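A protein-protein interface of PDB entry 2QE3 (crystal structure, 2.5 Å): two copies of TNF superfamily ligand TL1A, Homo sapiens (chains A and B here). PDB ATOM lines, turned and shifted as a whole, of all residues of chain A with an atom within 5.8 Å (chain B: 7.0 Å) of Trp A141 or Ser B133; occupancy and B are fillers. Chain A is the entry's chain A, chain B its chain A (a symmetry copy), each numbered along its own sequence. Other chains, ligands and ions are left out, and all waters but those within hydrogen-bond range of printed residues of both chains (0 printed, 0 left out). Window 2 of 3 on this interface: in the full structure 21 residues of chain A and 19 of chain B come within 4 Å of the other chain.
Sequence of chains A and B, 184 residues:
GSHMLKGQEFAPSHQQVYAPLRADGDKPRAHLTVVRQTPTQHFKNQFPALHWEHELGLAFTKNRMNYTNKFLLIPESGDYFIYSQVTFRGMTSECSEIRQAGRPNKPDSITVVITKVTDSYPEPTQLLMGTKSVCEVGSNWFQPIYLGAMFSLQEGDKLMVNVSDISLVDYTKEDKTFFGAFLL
The backbone NH (N) of Phe A142 sits at hydrogen-bond distance from the side-chain hydroxyl (OG) of Ser B133.
Cys A135 touches its own counterpart, Cys B135.
N of Gly A90 is in hydrogen-bond range of O of Trp A141, 2.7 Å away.
OG1 of Thr B131 sits at hydrogen-bond distance from O of Ile B110 (3.0 Å).
N of Ile B110 sits at hydrogen-bond distance from O of Lys B132.
The backbone NH of Phe A88 sits at hydrogen-bond distance from the backbone carbonyl oxygen of Gln A143 (2.5 Å).
The side-chain amino group of Lys B132 lies close to the side-chain amide oxygen of Gln B143 (3.4 Å).
Hydrophobic or aromatic side chains of chain A within 4 Å of the printed part of chain B: Val A137 and Phe A142.
Among the printed residues, no Asp or Glu carboxylate lies within 4 Å of a Lys or Arg side-chain nitrogen of the other chain.
Among the printed residues, merely in contact across the chains: Cys A135 with Cys B135 (3.6 Å), Val A137 with Cys B135 (3.7 Å), Trp A141 with Ser B133 (3.6 Å), Phe A142 with Thr B131 (3.4 Å), Phe A142 with Lys B132 (3.5 Å) and Gln A143 with Lys B132 (3.2 Å).
Printed residues of chain B within 4 Å of Trp A141: Ser B133 (3.6 Å).
Of the printed residues of chain A, Lys B132 touches Phe A142 and Gln A143.
Printed residues of chain B within 4 Å of Gln A143: Lys B132.
Of the printed residues of chain B, Cys A135 touches Cys B135.
Of the printed residues of chain B, Val A137 touches Cys B135.
Of the printed residues of chain A, Thr B131 touches Phe A142 (3.4 Å).
Gly A138 touches none of the printed residues of chain B.
Asn A140 touches none of the printed residues of chain B.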
ATOM      1  N   PHE A  88       9.937  34.410 -24.187  1.00  0.00           N
ATOM      2  CA  PHE A  88       8.921  34.321 -25.241  1.00  0.00           C
ATOM      3  C   PHE A  88       8.818  32.932 -25.730  1.00  0.00           C
ATOM      4  O   PHE A  88       9.840  32.297 -25.868  1.00  0.00           O
ATOM      5  CB  PHE A  88       9.330  35.107 -26.437  1.00  0.00           C
ATOM      6  CG  PHE A  88       9.309  36.586 -26.232  1.00  0.00           C
ATOM      7  CD1 PHE A  88       8.149  37.288 -26.297  1.00  0.00           C
ATOM      8  CD2 PHE A  88      10.465  37.278 -26.007  1.00  0.00           C
ATOM      9  CE1 PHE A  88       8.152  38.672 -26.116  1.00  0.00           C
ATOM     10  CE2 PHE A  88      10.471  38.668 -25.820  1.00  0.00           C
ATOM     11  CZ  PHE A  88       9.320  39.361 -25.861  1.00  0.00           C
ATOM     12  N   ARG A  89       7.608  32.460 -26.045  1.00  0.00           N
ATOM     13  CA  ARG A  89       7.436  31.138 -26.669  1.00  0.00           C
ATOM     14  C   ARG A  89       6.358  31.114 -27.761  1.00  0.00           C
ATOM     15  O   ARG A  89       5.391  31.901 -27.694  1.00  0.00           O
ATOM     16  CB  ARG A  89       7.132  30.070 -25.618  1.00  0.00           C
ATOM     17  CG  ARG A  89       5.876  30.317 -24.795  1.00  0.00           C
ATOM     18  CD  ARG A  89       5.691  29.255 -23.703  1.00  0.00           C
ATOM     19  NE  ARG A  89       4.307  29.287 -23.207  1.00  0.00           N
ATOM     20  CZ  ARG A  89       3.767  28.379 -22.395  1.00  0.00           C
ATOM     21  NH1 ARG A  89       4.504  27.356 -21.980  1.00  0.00           N
ATOM     22  NH2 ARG A  89       2.491  28.498 -22.011  1.00  0.00           N
ATOM     23  N   GLY A  90       6.513  30.201 -28.757  1.00  0.00           N
ATOM     24  CA  GLY A  90       5.598  30.104 -29.925  1.00  0.00           C
ATOM     25  C   GLY A  90       4.188  29.555 -29.717  1.00  0.00           C
ATOM     26  O   GLY A  90       4.009  28.544 -29.025  1.00  0.00           O
ATOM     27  N   LYS A 106       6.142  31.996 -37.382  1.00  0.00           N
ATOM     28  CA  LYS A 106       5.255  32.955 -38.115  1.00  0.00           C
ATOM     29  C   LYS A 106       5.358  34.440 -37.691  1.00  0.00           C
ATOM     30  O   LYS A 106       4.649  35.255 -38.265  1.00  0.00           O
ATOM     31  CB  LYS A 106       3.753  32.493 -38.166  1.00  0.00           C
ATOM     32  CG  LYS A 106       3.678  30.961 -38.328  1.00  0.00           C
ATOM     33  CD  LYS A 106       2.307  30.371 -38.094  1.00  0.00           C
ATOM     34  CE  LYS A 106       1.576  30.140 -39.428  1.00  0.00           C
ATOM     35  NZ  LYS A 106       1.009  31.447 -39.934  1.00  0.00           N
ATOM     36  N   PRO A 107       6.170  34.801 -36.656  1.00  0.00           N
ATOM     37  CA  PRO A 107       6.628  36.219 -36.518  1.00  0.00           C
ATOM     38  C   PRO A 107       8.111  36.499 -36.859  1.00  0.00           C
ATOM     39  O   PRO A 107       8.941  35.573 -36.992  1.00  0.00           O
ATOM     40  CB  PRO A 107       6.405  36.508 -35.046  1.00  0.00           C
ATOM     41  CG  PRO A 107       6.673  35.133 -34.416  1.00  0.00           C
ATOM     42  CD  PRO A 107       6.568  34.025 -35.472  1.00  0.00           C
ATOM     43  N   ILE A 110      11.161  39.166 -31.871  1.00  0.00           N
ATOM     44  CA  ILE A 110      10.707  39.558 -30.563  1.00  0.00           C
ATOM     45  C   ILE A 110      11.518  40.718 -29.959  1.00  0.00           C
ATOM     46  O   ILE A 110      12.694  40.899 -30.244  1.00  0.00           O
ATOM     47  CB  ILE A 110      10.818  38.404 -29.615  1.00  0.00           C
ATOM     48  CG1 ILE A 110      12.191  37.809 -29.769  1.00  0.00           C
ATOM     49  CG2 ILE A 110       9.813  37.384 -29.921  1.00  0.00           C
ATOM     50  CD1 ILE A 110      12.218  36.421 -29.294  1.00  0.00           C
ATOM     51  N   VAL A 134      13.604  35.827 -34.897  1.00  0.00           N
ATOM     52  CA  VAL A 134      13.188  34.425 -34.591  1.00  0.00           C
ATOM     53  C   VAL A 134      13.399  33.338 -35.699  1.00  0.00           C
ATOM     54  O   VAL A 134      13.194  33.594 -36.906  1.00  0.00           O
ATOM     55  CB  VAL A 134      11.753  34.358 -34.070  1.00  0.00           C
ATOM     56  CG1 VAL A 134      11.740  33.548 -32.769  1.00  0.00           C
ATOM     57  CG2 VAL A 134      11.212  35.773 -33.858  1.00  0.00           C
ATOM     58  N   CYS A 135      13.814  32.138 -35.245  1.00  0.00           N
ATOM     59  CA  CYS A 135      14.182  30.964 -36.083  1.00  0.00           C
ATOM     60  C   CYS A 135      13.125  29.877 -36.105  1.00  0.00           C
ATOM     61  O   CYS A 135      12.997  29.093 -35.160  1.00  0.00           O
ATOM     62  CB  CYS A 135      15.476  30.333 -35.596  1.00  0.00           C
ATOM     63  SG  CYS A 135      16.812  30.559 -36.732  1.00  0.00           S
ATOM     64  N   GLU A 136      12.433  29.789 -37.232  1.00  0.00           N
ATOM     65  CA  GLU A 136      11.108  29.167 -37.305  1.00  0.00           C
ATOM     66  C   GLU A 136      11.095  27.596 -37.375  1.00  0.00           C
ATOM     67  O   GLU A 136      10.371  26.956 -38.156  1.00  0.00           O
ATOM     68  CB  GLU A 136      10.249  29.919 -38.361  1.00  0.00           C
ATOM     69  CG  GLU A 136      10.993  30.466 -39.667  1.00  0.00           C
ATOM     70  CD  GLU A 136      12.067  31.605 -39.476  1.00  0.00           C
ATOM     71  OE1 GLU A 136      13.195  31.302 -39.021  1.00  0.00           O
ATOM     72  OE2 GLU A 136      11.813  32.780 -39.853  1.00  0.00           O
ATOM     73  N   VAL A 137      11.899  27.016 -36.482  1.00  0.00           N
ATOM     74  CA  VAL A 137      12.084  25.575 -36.281  1.00  0.00           C
ATOM     75  C   VAL A 137      11.149  25.030 -35.192  1.00  0.00           C
ATOM     76  O   VAL A 137      11.419  25.175 -33.989  1.00  0.00           O
ATOM     77  CB  VAL A 137      13.541  25.297 -35.815  1.00  0.00           C
ATOM     78  CG1 VAL A 137      13.731  23.836 -35.353  1.00  0.00           C
ATOM     79  CG2 VAL A 137      14.528  25.673 -36.904  1.00  0.00           C
ATOM     80  N   GLY A 138      10.066  24.382 -35.608  1.00  0.00           N
ATOM     81  CA  GLY A 138       9.091  23.837 -34.661  1.00  0.00           C
ATOM     82  C   GLY A 138       7.716  23.725 -35.298  1.00  0.00           C
ATOM     83  O   GLY A 138       7.334  22.650 -35.766  1.00  0.00           O
ATOM     84  N   SER A 139       6.951  24.816 -35.280  1.00  0.00           N
ATOM     85  CA  SER A 139       7.327  25.972 -34.496  1.00  0.00           C
ATOM     86  C   SER A 139       6.614  26.059 -33.095  1.00  0.00           C
ATOM     87  O   SER A 139       5.674  26.852 -32.852  1.00  0.00           O
ATOM     88  CB  SER A 139       7.423  27.271 -35.354  1.00  0.00           C
ATOM     89  OG  SER A 139       6.192  27.852 -35.737  1.00  0.00           O
ATOM     90  N   ASN A 140       7.066  25.160 -32.208  1.00  0.00           N
ATOM     91  CA  ASN A 140       7.006  25.367 -30.757  1.00  0.00           C
ATOM     92  C   ASN A 140       8.422  25.770 -30.277  1.00  0.00           C
ATOM     93  O   ASN A 140       9.250  24.924 -29.999  1.00  0.00           O
ATOM     94  CB  ASN A 140       6.496  24.117 -29.995  1.00  0.00           C
ATOM     95  CG  ASN A 140       6.337  24.372 -28.463  1.00  0.00           C
ATOM     96  OD1 ASN A 140       6.796  23.567 -27.614  1.00  0.00           O
ATOM     97  ND2 ASN A 140       5.695  25.514 -28.114  1.00  0.00           N
ATOM     98  N   TRP A 141       8.700  27.069 -30.209  1.00  0.00           N
ATOM     99  CA  TRP A 141      10.002  27.563 -29.795  1.00  0.00           C
ATOM    100  C   TRP A 141       9.825  28.425 -28.552  1.00  0.00           C
ATOM    101  O   TRP A 141       8.691  28.766 -28.189  1.00  0.00           O
ATOM    102  CB  TRP A 141      10.588  28.375 -30.912  1.00  0.00           C
ATOM    103  CG  TRP A 141       9.664  29.471 -31.307  1.00  0.00           C
ATOM    104  CD1 TRP A 141       8.725  29.439 -32.280  1.00  0.00           C
ATOM    105  CD2 TRP A 141       9.578  30.767 -30.725  1.00  0.00           C
ATOM    106  NE1 TRP A 141       8.054  30.624 -32.340  1.00  0.00           N
ATOM    107  CE2 TRP A 141       8.556  31.450 -31.379  1.00  0.00           C
ATOM    108  CE3 TRP A 141      10.258  31.409 -29.688  1.00  0.00           C
ATOM    109  CZ2 TRP A 141       8.197  32.737 -31.037  1.00  0.00           C
ATOM    110  CZ3 TRP A 141       9.902  32.666 -29.352  1.00  0.00           C
ATOM    111  CH2 TRP A 141       8.888  33.332 -30.026  1.00  0.00           C
ATOM    112  N   PHE A 142      10.944  28.758 -27.905  1.00  0.00           N
ATOM    113  CA  PHE A 142      10.996  29.787 -26.872  1.00  0.00           C
ATOM    114  C   PHE A 142      12.394  30.321 -26.667  1.00  0.00           C
ATOM    115  O   PHE A 142      13.427  29.651 -26.757  1.00  0.00           O
ATOM    116  CB  PHE A 142      10.450  29.306 -25.529  1.00  0.00           C
ATOM    117  CG  PHE A 142      10.863  27.917 -25.172  1.00  0.00           C
ATOM    118  CD1 PHE A 142       9.988  26.853 -25.347  1.00  0.00           C
ATOM    119  CD2 PHE A 142      12.111  27.660 -24.702  1.00  0.00           C
ATOM    120  CE1 PHE A 142      10.343  25.534 -25.033  1.00  0.00           C
ATOM    121  CE2 PHE A 142      12.488  26.337 -24.409  1.00  0.00           C
ATOM    122  CZ  PHE A 142      11.591  25.272 -24.575  1.00  0.00           C
ATOM    123  N   GLN A 143      12.398  31.595 -26.387  1.00  0.00           N
ATOM    124  CA  GLN A 143      13.596  32.358 -26.163  1.00  0.00           C
ATOM    125  C   GLN A 143      13.342  33.267 -24.982  1.00  0.00           C
ATOM    126  O   GLN A 143      12.265  33.912 -24.907  1.00  0.00           O
ATOM    127  CB  GLN A 143      13.863  33.203 -27.382  1.00  0.00           C
ATOM    128  CG  GLN A 143      14.595  32.448 -28.394  1.00  0.00           C
ATOM    129  CD  GLN A 143      16.044  32.521 -28.100  1.00  0.00           C
ATOM    130  OE1 GLN A 143      16.467  33.417 -27.349  1.00  0.00           O
ATOM    131  NE2 GLN A 143      16.844  31.610 -28.694  1.00  0.00           N
ATOM    132  N   LEU A 168       2.861  36.331 -27.063  1.00  0.00           N
ATOM    133  CA  LEU A 168       4.027  35.431 -27.075  1.00  0.00           C
ATOM    134  C   LEU A 168       4.697  35.184 -25.758  1.00  0.00           C
ATOM    135  O   LEU A 168       5.621  34.379 -25.656  1.00  0.00           O
ATOM    136  CB  LEU A 168       5.085  35.905 -28.079  1.00  0.00           C
ATOM    137  CG  LEU A 168       4.271  35.712 -29.348  1.00  0.00           C
ATOM    138  CD1 LEU A 168       4.972  36.288 -30.518  1.00  0.00           C
ATOM    139  CD2 LEU A 168       3.920  34.245 -29.563  1.00  0.00           C
ATOM    140  N   PRO B 107      19.465  17.623 -29.000  1.00  0.00           N
ATOM    141  CA  PRO B 107      18.511  17.936 -27.889  1.00  0.00           C
ATOM    142  C   PRO B 107      17.447  19.020 -28.181  1.00  0.00           C
ATOM    143  O   PRO B 107      17.530  19.770 -29.178  1.00  0.00           O
ATOM    144  CB  PRO B 107      19.424  18.436 -26.786  1.00  0.00           C
ATOM    145  CG  PRO B 107      20.536  19.124 -27.592  1.00  0.00           C
ATOM    146  CD  PRO B 107      20.533  18.632 -29.045  1.00  0.00           C
ATOM    147  N   ASP B 108      16.463  19.106 -27.293  1.00  0.00           N
ATOM    148  CA  ASP B 108      15.331  19.959 -27.555  1.00  0.00           C
ATOM    149  C   ASP B 108      15.522  21.374 -27.078  1.00  0.00           C
ATOM    150  O   ASP B 108      15.173  22.364 -27.757  1.00  0.00           O
ATOM    151  CB  ASP B 108      14.093  19.369 -26.912  1.00  0.00           C
ATOM    152  CG  ASP B 108      13.141  18.803 -27.941  1.00  0.00           C
ATOM    153  OD1 ASP B 108      13.280  19.179 -29.136  1.00  0.00           O
ATOM    154  OD2 ASP B 108      12.257  17.995 -27.561  1.00  0.00           O
ATOM    155  N   SER B 109      16.087  21.454 -25.888  1.00  0.00           N
ATOM    156  CA  SER B 109      16.186  22.701 -25.215  1.00  0.00           C
ATOM    157  C   SER B 109      17.323  22.646 -24.248  1.00  0.00           C
ATOM    158  O   SER B 109      17.726  21.581 -23.790  1.00  0.00           O
ATOM    159  CB  SER B 109      14.880  22.990 -24.461  1.00  0.00           C
ATOM    160  OG  SER B 109      14.652  22.014 -23.447  1.00  0.00           O
ATOM    161  N   ILE B 110      17.820  23.824 -23.929  1.00  0.00           N
ATOM    162  CA  ILE B 110      18.666  24.033 -22.785  1.00  0.00           C
ATOM    163  C   ILE B 110      18.016  24.907 -21.698  1.00  0.00           C
ATOM    164  O   ILE B 110      17.187  25.764 -21.971  1.00  0.00           O
ATOM    165  CB  ILE B 110      19.931  24.718 -23.202  1.00  0.00           C
ATOM    166  CG1 ILE B 110      19.559  25.893 -24.065  1.00  0.00           C
ATOM    167  CG2 ILE B 110      20.785  23.807 -23.968  1.00  0.00           C
ATOM    168  CD1 ILE B 110      20.683  26.297 -24.914  1.00  0.00           C
ATOM    169  N   THR B 131      15.279  29.278 -20.023  1.00  0.00           N
ATOM    170  CA  THR B 131      15.127  28.168 -20.952  1.00  0.00           C
ATOM    171  C   THR B 131      15.015  28.579 -22.439  1.00  0.00           C
ATOM    172  O   THR B 131      14.299  29.514 -22.801  1.00  0.00           O
ATOM    173  CB  THR B 131      14.064  27.189 -20.470  1.00  0.00           C
ATOM    174  OG1 THR B 131      14.382  25.899 -20.951  1.00  0.00           O
ATOM    175  CG2 THR B 131      12.633  27.543 -20.845  1.00  0.00           C
ATOM    176  N   LYS B 132      15.787  27.910 -23.268  1.00  0.00           N
ATOM    177  CA  LYS B 132      15.864  28.221 -24.682  1.00  0.00           C
ATOM    178  C   LYS B 132      15.766  26.927 -25.476  1.00  0.00           C
ATOM    179  O   LYS B 132      16.319  25.903 -25.075  1.00  0.00           O
ATOM    180  CB  LYS B 132      17.206  28.826 -24.973  1.00  0.00           C
ATOM    181  CG  LYS B 132      17.390  29.561 -26.275  1.00  0.00           C
ATOM    182  CD  LYS B 132      18.732  30.436 -26.233  1.00  0.00           C
ATOM    183  CE  LYS B 132      18.566  31.670 -25.238  1.00  0.00           C
ATOM    184  NZ  LYS B 132      19.550  32.810 -25.200  1.00  0.00           N
ATOM    185  N   SER B 133      15.048  26.981 -26.596  1.00  0.00           N
ATOM    186  CA  SER B 133      14.968  25.842 -27.485  1.00  0.00           C
ATOM    187  C   SER B 133      16.206  25.956 -28.330  1.00  0.00           C
ATOM    188  O   SER B 133      16.727  27.073 -28.508  1.00  0.00           O
ATOM    189  CB  SER B 133      13.708  25.914 -28.350  1.00  0.00           C
ATOM    190  OG  SER B 133      12.547  26.268 -27.587  1.00  0.00           O
ATOM    191  N   VAL B 134      16.667  24.804 -28.827  1.00  0.00           N
ATOM    192  CA  VAL B 134      17.889  24.744 -29.685  1.00  0.00           C
ATOM    193  C   VAL B 134      17.696  24.497 -31.220  1.00  0.00           C
ATOM    194  O   VAL B 134      16.832  23.700 -31.645  1.00  0.00           O
ATOM    195  CB  VAL B 134      18.925  23.767 -29.133  1.00  0.00           C
ATOM    196  CG1 VAL B 134      20.279  24.482 -29.050  1.00  0.00           C
ATOM    197  CG2 VAL B 134      18.476  23.253 -27.764  1.00  0.00           C
ATOM    198  N   CYS B 135      18.521  25.208 -32.017  1.00  0.00           N
ATOM    199  CA  CYS B 135      18.489  25.239 -33.505  1.00  0.00           C
ATOM    200  C   CYS B 135      19.595  24.430 -34.154  1.00  0.00           C
ATOM    201  O   CYS B 135      20.748  24.868 -34.224  1.00  0.00           O
ATOM    202  CB  CYS B 135      18.601  26.664 -34.020  1.00  0.00           C
ATOM    203  SG  CYS B 135      17.105  27.236 -34.769  1.00  0.00           S
ATOM    204  N   GLN B 143      25.396  28.396 -27.186  1.00  0.00           N
ATOM    205  CA  GLN B 143      24.552  29.460 -26.714  1.00  0.00           C
ATOM    206  C   GLN B 143      24.918  29.724 -25.271  1.00  0.00           C
ATOM    207  O   GLN B 143      25.075  28.762 -24.477  1.00  0.00           O
ATOM    208  CB  GLN B 143      23.118  29.002 -26.779  1.00  0.00           C
ATOM    209  CG  GLN B 143      22.558  29.217 -28.109  1.00  0.00           C
ATOM    210  CD  GLN B 143      22.055  30.607 -28.205  1.00  0.00           C
ATOM    211  OE1 GLN B 143      21.835  31.246 -27.161  1.00  0.00           O
ATOM    212  NE2 GLN B 143      21.835  31.103 -29.440  1.00  0.00           N
